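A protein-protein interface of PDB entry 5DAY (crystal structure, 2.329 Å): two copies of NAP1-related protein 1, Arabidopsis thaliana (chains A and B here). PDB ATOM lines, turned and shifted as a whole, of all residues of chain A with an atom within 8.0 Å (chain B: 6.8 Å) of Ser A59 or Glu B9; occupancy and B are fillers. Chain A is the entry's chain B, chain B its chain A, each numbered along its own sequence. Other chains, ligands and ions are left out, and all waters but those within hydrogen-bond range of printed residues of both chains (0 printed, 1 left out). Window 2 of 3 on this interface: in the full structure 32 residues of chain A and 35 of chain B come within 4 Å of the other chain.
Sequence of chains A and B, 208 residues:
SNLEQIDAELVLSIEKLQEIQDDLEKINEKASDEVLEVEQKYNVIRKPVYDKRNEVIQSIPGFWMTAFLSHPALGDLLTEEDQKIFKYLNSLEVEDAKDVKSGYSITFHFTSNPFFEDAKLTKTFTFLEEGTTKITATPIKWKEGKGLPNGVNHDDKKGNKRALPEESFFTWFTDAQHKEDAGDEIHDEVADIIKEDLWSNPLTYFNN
The side-chain carboxylate (OE2) of Glu B9 lies within hydrogen-bond range of the side-chain amide nitrogen (NE2) of Gln B5. The backbone carbonyl oxygen (O) of Glu B9 lies within hydrogen-bond range of the side-chain hydroxyl (OG) of Ser B13 (3.3 Å).
No position is printed for both chains. Of the 7 pairs that touch across the chains among the printed residues, none has its exchanged pair printed and touching as well.
Among the printed residues, pairs that only touch across the chains: Ser A59 with Ser B13 (3.2 Å), Val A56 with Ser B13 (3.3 Å), Ser A59 with Leu B10 (3.9 Å), Ile A60 with Ser B13 (3.9 Å), Pro A61 with Leu B10 (3.98 Å) and Ile A60 with Ile B14 (3.997 Å).
Ser A59 touches just these residues of chain B: Glu B9 (3.4 Å), Leu B10 (3.9 Å) and Ser B13 (3.2 Å). Of chain A, only Ser A59 (3.4 Å) comes within 4 Å of Glu B9. No residue of chain A comes within 4 Å of Ala B8. Printed residues of chain A within 4 Å of Leu B10: Ser A59 and Pro A61. Of the printed residues of chain B, Pro A61 touches Leu B10 (3.98 Å). The nearest residue of chain B that does not touch Ser A59 is Ile B6 (5.4 Å). The nearest printed residue of chain B that does not touch Ile A60 is Leu B10 (4.1 Å).
OE1 of Glu B9 is in hydrogen-bond range of OG of Ser A59, at 3.4 Å.
Of the 11 printed residues of chain A, 4 touch a printed residue of chain B. Hydrophobic or aromatic side chains of chain A that line the printed part of chain B: Val A56, Ile A60 and Pro A61. Of the 11 printed residues of chain B, 4 touch a printed residue of chain A. Among the printed residues, no Asp or Glu carboxylate lies within 4 Å of a Lys or Arg side-chain nitrogen of the other chain.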
ATOM      1  N   ARG A  53      -3.792  -8.812   2.231  1.00  0.00           N
ATOM      2  CA  ARG A  53      -3.808  -9.709   1.079  1.00  0.00           C
ATOM      3  C   ARG A  53      -2.801  -9.266   0.016  1.00  0.00           C
ATOM      4  O   ARG A  53      -2.096 -10.100  -0.570  1.00  0.00           O
ATOM      5  CB  ARG A  53      -5.200  -9.793   0.474  1.00  0.00           C
ATOM      6  CG  ARG A  53      -5.372 -10.964  -0.465  1.00  0.00           C
ATOM      7  CD  ARG A  53      -6.776 -11.015  -1.045  1.00  0.00           C
ATOM      8  NE  ARG A  53      -7.047  -9.897  -1.949  1.00  0.00           N
ATOM      9  CZ  ARG A  53      -8.160  -9.764  -2.666  1.00  0.00           C
ATOM     10  NH1 ARG A  53      -9.116 -10.682  -2.587  1.00  0.00           N
ATOM     11  NH2 ARG A  53      -8.316  -8.719  -3.469  1.00  0.00           N
ATOM     12  N   ASN A  54      -2.718  -7.955  -0.237  1.00  0.00           N
ATOM     13  CA  ASN A  54      -1.748  -7.436  -1.195  1.00  0.00           C
ATOM     14  C   ASN A  54      -0.319  -7.754  -0.753  1.00  0.00           C
ATOM     15  O   ASN A  54       0.528  -8.130  -1.575  1.00  0.00           O
ATOM     16  CB  ASN A  54      -1.951  -5.926  -1.360  1.00  0.00           C
ATOM     17  CG  ASN A  54      -1.067  -5.318  -2.444  1.00  0.00           C
ATOM     18  OD1 ASN A  54      -0.877  -5.902  -3.515  1.00  0.00           O
ATOM     19  ND2 ASN A  54      -0.521  -4.132  -2.169  1.00  0.00           N
ATOM     20  N   GLU A  55      -0.036  -7.625   0.548  1.00  0.00           N
ATOM     21  CA  GLU A  55       1.309  -7.903   1.040  1.00  0.00           C
ATOM     22  C   GLU A  55       1.694  -9.359   0.795  1.00  0.00           C
ATOM     23  O   GLU A  55       2.752  -9.643   0.230  1.00  0.00           O
ATOM     24  CB  GLU A  55       1.415  -7.547   2.526  1.00  0.00           C
ATOM     25  CG  GLU A  55       2.673  -8.095   3.186  1.00  0.00           C
ATOM     26  CD  GLU A  55       3.067  -7.381   4.475  1.00  0.00           C
ATOM     27  OE1 GLU A  55       2.378  -6.420   4.875  1.00  0.00           O
ATOM     28  OE2 GLU A  55       4.091  -7.777   5.088  1.00  0.00           O
ATOM     29  N   VAL A  56       0.831 -10.294   1.203  1.00  0.00           N
ATOM     30  CA  VAL A  56       1.077 -11.725   1.030  1.00  0.00           C
ATOM     31  C   VAL A  56       1.264 -12.083  -0.439  1.00  0.00           C
ATOM     32  O   VAL A  56       2.098 -12.935  -0.780  1.00  0.00           O
ATOM     33  CB  VAL A  56      -0.082 -12.516   1.679  1.00  0.00           C
ATOM     34  CG1 VAL A  56      -0.182 -13.930   1.129  1.00  0.00           C
ATOM     35  CG2 VAL A  56       0.088 -12.540   3.192  1.00  0.00           C
ATOM     36  N   ILE A  57       0.518 -11.424  -1.332  1.00  0.00           N
ATOM     37  CA  ILE A  57       0.576 -11.720  -2.760  1.00  0.00           C
ATOM     38  C   ILE A  57       1.956 -11.432  -3.359  1.00  0.00           C
ATOM     39  O   ILE A  57       2.321 -12.029  -4.380  1.00  0.00           O
ATOM     40  CB  ILE A  57      -0.565 -10.941  -3.481  1.00  0.00           C
ATOM     41  CG1 ILE A  57      -1.902 -11.659  -3.279  1.00  0.00           C
ATOM     42  CG2 ILE A  57      -0.311 -10.774  -4.981  1.00  0.00           C
ATOM     43  CD1 ILE A  57      -3.137 -10.887  -3.805  1.00  0.00           C
ATOM     44  N   GLN A  58       2.747 -10.544  -2.741  1.00  0.00           N
ATOM     45  CA  GLN A  58       4.086 -10.239  -3.259  1.00  0.00           C
ATOM     46  C   GLN A  58       4.997 -11.454  -3.273  1.00  0.00           C
ATOM     47  O   GLN A  58       5.985 -11.454  -4.011  1.00  0.00           O
ATOM     48  CB  GLN A  58       4.774  -9.139  -2.442  1.00  0.00           C
ATOM     49  CG  GLN A  58       3.930  -7.891  -2.291  1.00  0.00           C
ATOM     50  CD  GLN A  58       3.439  -7.384  -3.633  1.00  0.00           C
ATOM     51  OE1 GLN A  58       4.223  -7.239  -4.573  1.00  0.00           O
ATOM     52  NE2 GLN A  58       2.137  -7.128  -3.738  1.00  0.00           N
ATOM     53  N   SER A  59       4.700 -12.479  -2.476  1.00  0.00           N
ATOM     54  CA  SER A  59       5.557 -13.658  -2.407  1.00  0.00           C
ATOM     55  C   SER A  59       5.102 -14.769  -3.333  1.00  0.00           C
ATOM     56  O   SER A  59       5.700 -15.850  -3.325  1.00  0.00           O
ATOM     57  CB  SER A  59       5.628 -14.181  -0.970  1.00  0.00           C
ATOM     58  OG  SER A  59       6.188 -13.205  -0.102  1.00  0.00           O
ATOM     59  N   ILE A  60       4.074 -14.531  -4.138  1.00  0.00           N
ATOM     60  CA  ILE A  60       3.543 -15.544  -5.040  1.00  0.00           C
ATOM     61  C   ILE A  60       3.747 -15.049  -6.471  1.00  0.00           C
ATOM     62  O   ILE A  60       3.056 -14.118  -6.908  1.00  0.00           O
ATOM     63  CB  ILE A  60       2.069 -15.840  -4.747  1.00  0.00           C
ATOM     64  CG1 ILE A  60       1.892 -16.107  -3.253  1.00  0.00           C
ATOM     65  CG2 ILE A  60       1.622 -17.025  -5.546  1.00  0.00           C
ATOM     66  CD1 ILE A  60       0.453 -16.291  -2.803  1.00  0.00           C
ATOM     67  N   PRO A  61       4.667 -15.636  -7.236  1.00  0.00           N
ATOM     68  CA  PRO A  61       4.980 -15.089  -8.563  1.00  0.00           C
ATOM     69  C   PRO A  61       3.806 -15.203  -9.529  1.00  0.00           C
ATOM     70  O   PRO A  61       3.129 -16.232  -9.603  1.00  0.00           O
ATOM     71  CB  PRO A  61       6.175 -15.939  -9.026  1.00  0.00           C
ATOM     72  CG  PRO A  61       6.039 -17.235  -8.256  1.00  0.00           C
ATOM     73  CD  PRO A  61       5.410 -16.874  -6.938  1.00  0.00           C
ATOM     74  N   GLY A  62       3.573 -14.126 -10.274  1.00  0.00           N
ATOM     75  CA  GLY A  62       2.559 -14.128 -11.309  1.00  0.00           C
ATOM     76  C   GLY A  62       1.167 -14.438 -10.811  1.00  0.00           C
ATOM     77  O   GLY A  62       0.370 -15.029 -11.545  1.00  0.00           O
ATOM     78  N   PHE A  63       0.855 -14.052  -9.573  1.00  0.00           N
ATOM     79  CA  PHE A  63      -0.429 -14.413  -8.979  1.00  0.00           C
ATOM     80  C   PHE A  63      -1.595 -13.807  -9.751  1.00  0.00           C
ATOM     81  O   PHE A  63      -2.466 -14.523 -10.258  1.00  0.00           O
ATOM     82  CB  PHE A  63      -0.481 -13.964  -7.518  1.00  0.00           C
ATOM     83  CG  PHE A  63      -1.811 -14.182  -6.892  1.00  0.00           C
ATOM     84  CD1 PHE A  63      -2.164 -15.436  -6.415  1.00  0.00           C
ATOM     85  CD2 PHE A  63      -2.738 -13.151  -6.818  1.00  0.00           C
ATOM     86  CE1 PHE A  63      -3.425 -15.659  -5.848  1.00  0.00           C
ATOM     87  CE2 PHE A  63      -3.992 -13.368  -6.262  1.00  0.00           C
ATOM     88  CZ  PHE A  63      -4.334 -14.634  -5.774  1.00  0.00           C
ATOM     89  N   GLU B   4      16.031 -21.213  -0.995  1.00  0.00           N
ATOM     90  CA  GLU B   4      15.256 -22.027  -0.060  1.00  0.00           C
ATOM     91  C   GLU B   4      14.292 -21.176   0.743  1.00  0.00           C
ATOM     92  O   GLU B   4      13.165 -21.600   1.040  1.00  0.00           O
ATOM     93  CB  GLU B   4      16.181 -22.772   0.896  1.00  0.00           C
ATOM     94  CG  GLU B   4      17.136 -23.737   0.238  1.00  0.00           C
ATOM     95  CD  GLU B   4      18.341 -24.063   1.132  1.00  0.00           C
ATOM     96  OE1 GLU B   4      18.950 -23.118   1.700  1.00  0.00           O
ATOM     97  OE2 GLU B   4      18.682 -25.263   1.270  1.00  0.00           O
ATOM     98  N   GLN B   5      14.732 -19.987   1.149  1.00  0.00           N
ATOM     99  CA  GLN B   5      13.855 -19.114   1.916  1.00  0.00           C
ATOM    100  C   GLN B   5      12.693 -18.631   1.058  1.00  0.00           C
ATOM    101  O   GLN B   5      11.551 -18.548   1.531  1.00  0.00           O
ATOM    102  CB  GLN B   5      14.656 -17.938   2.481  1.00  0.00           C
ATOM    103  CG  GLN B   5      13.843 -16.909   3.257  1.00  0.00           C
ATOM    104  CD  GLN B   5      13.672 -15.615   2.466  1.00  0.00           C
ATOM    105  OE1 GLN B   5      14.596 -15.176   1.769  1.00  0.00           O
ATOM    106  NE2 GLN B   5      12.482 -15.014   2.549  1.00  0.00           N
ATOM    107  N   ILE B   6      12.959 -18.309  -0.211  1.00  0.00           N
ATOM    108  CA  ILE B   6      11.876 -17.867  -1.076  1.00  0.00           C
ATOM    109  C   ILE B   6      10.908 -19.015  -1.335  1.00  0.00           C
ATOM    110  O   ILE B   6       9.682 -18.830  -1.302  1.00  0.00           O
ATOM    111  CB  ILE B   6      12.433 -17.265  -2.377  1.00  0.00           C
ATOM    112  CG1 ILE B   6      13.038 -15.894  -2.066  1.00  0.00           C
ATOM    113  CG2 ILE B   6      11.311 -17.068  -3.373  1.00  0.00           C
ATOM    114  CD1 ILE B   6      14.180 -15.503  -2.975  1.00  0.00           C
ATOM    115  N   ASP B   7      11.450 -20.222  -1.545  1.00  0.00           N
ATOM    116  CA  ASP B   7      10.630 -21.413  -1.716  1.00  0.00           C
ATOM    117  C   ASP B   7       9.699 -21.612  -0.515  1.00  0.00           C
ATOM    118  O   ASP B   7       8.464 -21.683  -0.665  1.00  0.00           O
ATOM    119  CB  ASP B   7      11.548 -22.605  -1.935  1.00  0.00           C
ATOM    120  CG  ASP B   7      10.804 -23.915  -2.165  1.00  0.00           C
ATOM    121  OD1 ASP B   7      10.098 -24.028  -3.193  1.00  0.00           O
ATOM    122  OD2 ASP B   7      10.997 -24.867  -1.355  1.00  0.00           O
ATOM    123  N   ALA B   8      10.274 -21.636   0.693  1.00  0.00           N
ATOM    124  CA  ALA B   8       9.476 -21.812   1.906  1.00  0.00           C
ATOM    125  C   ALA B   8       8.473 -20.681   2.070  1.00  0.00           C
ATOM    126  O   ALA B   8       7.317 -20.918   2.447  1.00  0.00           O
ATOM    127  CB  ALA B   8      10.379 -21.907   3.140  1.00  0.00           C
ATOM    128  N   GLU B   9       8.877 -19.456   1.786  1.00  0.00           N
ATOM    129  CA  GLU B   9       7.955 -18.340   1.835  1.00  0.00           C
ATOM    130  C   GLU B   9       6.801 -18.488   0.881  1.00  0.00           C
ATOM    131  O   GLU B   9       5.718 -18.091   1.179  1.00  0.00           O
ATOM    132  CB  GLU B   9       8.650 -17.039   1.549  1.00  0.00           C
ATOM    133  CG  GLU B   9       8.400 -16.001   2.562  1.00  0.00           C
ATOM    134  CD  GLU B   9       9.078 -14.688   2.262  1.00  0.00           C
ATOM    135  OE1 GLU B   9       9.225 -14.350   1.062  1.00  0.00           O
ATOM    136  OE2 GLU B   9       9.452 -13.984   3.218  1.00  0.00           O
ATOM    137  N   LEU B  10       7.046 -19.049  -0.284  1.00  0.00           N
ATOM    138  CA  LEU B  10       5.988 -19.234  -1.274  1.00  0.00           C
ATOM    139  C   LEU B  10       4.915 -20.192  -0.763  1.00  0.00           C
ATOM    140  O   LEU B  10       3.718 -19.907  -0.869  1.00  0.00           O
ATOM    141  CB  LEU B  10       6.605 -19.733  -2.585  1.00  0.00           C
ATOM    142  CG  LEU B  10       5.718 -20.371  -3.656  1.00  0.00           C
ATOM    143  CD1 LEU B  10       4.542 -19.460  -4.042  1.00  0.00           C
ATOM    144  CD2 LEU B  10       6.589 -20.680  -4.856  1.00  0.00           C
ATOM    145  N   VAL B  11       5.341 -21.330  -0.207  1.00  0.00           N
ATOM    146  CA  VAL B  11       4.421 -22.327   0.339  1.00  0.00           C
ATOM    147  C   VAL B  11       3.593 -21.724   1.474  1.00  0.00           C
ATOM    148  O   VAL B  11       2.360 -21.826   1.500  1.00  0.00           O
ATOM    149  CB  VAL B  11       5.223 -23.561   0.792  1.00  0.00           C
ATOM    150  CG1 VAL B  11       4.324 -24.620   1.445  1.00  0.00           C
ATOM    151  CG2 VAL B  11       5.995 -24.136  -0.384  1.00  0.00           C
ATOM    152  N   LEU B  12       4.268 -21.027   2.389  1.00  0.00           N
ATOM    153  CA  LEU B  12       3.614 -20.338   3.494  1.00  0.00           C
ATOM    154  C   LEU B  12       2.630 -19.275   3.007  1.00  0.00           C
ATOM    155  O   LEU B  12       1.537 -19.122   3.571  1.00  0.00           O
ATOM    156  CB  LEU B  12       4.694 -19.716   4.381  1.00  0.00           C
ATOM    157  CG  LEU B  12       4.354 -18.710   5.471  1.00  0.00           C
ATOM    158  CD1 LEU B  12       3.668 -19.397   6.657  1.00  0.00           C
ATOM    159  CD2 LEU B  12       5.629 -18.003   5.919  1.00  0.00           C
ATOM    160  N   SER B  13       3.002 -18.518   1.971  1.00  0.00           N
ATOM    161  CA  SER B  13       2.160 -17.413   1.521  1.00  0.00           C
ATOM    162  C   SER B  13       0.865 -17.909   0.890  1.00  0.00           C
ATOM    163  O   SER B  13      -0.167 -17.252   1.017  1.00  0.00           O
ATOM    164  CB  SER B  13       2.924 -16.523   0.535  1.00  0.00           C
ATOM    165  OG  SER B  13       3.695 -15.544   1.212  1.00  0.00           O
ATOM    166  N   ILE B  14       0.895 -19.062   0.225  1.00  0.00           N
ATOM    167  CA  ILE B  14      -0.335 -19.618  -0.334  1.00  0.00           C
ATOM    168  C   ILE B  14      -1.311 -20.000   0.779  1.00  0.00           C
ATOM    169  O   ILE B  14      -2.519 -19.742   0.679  1.00  0.00           O
ATOM    170  CB  ILE B  14      -0.006 -20.805  -1.258  1.00  0.00           C
ATOM    171  CG1 ILE B  14       0.454 -20.284  -2.618  1.00  0.00           C
ATOM    172  CG2 ILE B  14      -1.214 -21.713  -1.437  1.00  0.00           C
ATOM    173  CD1 ILE B  14       1.230 -21.307  -3.409  1.00  0.00           C
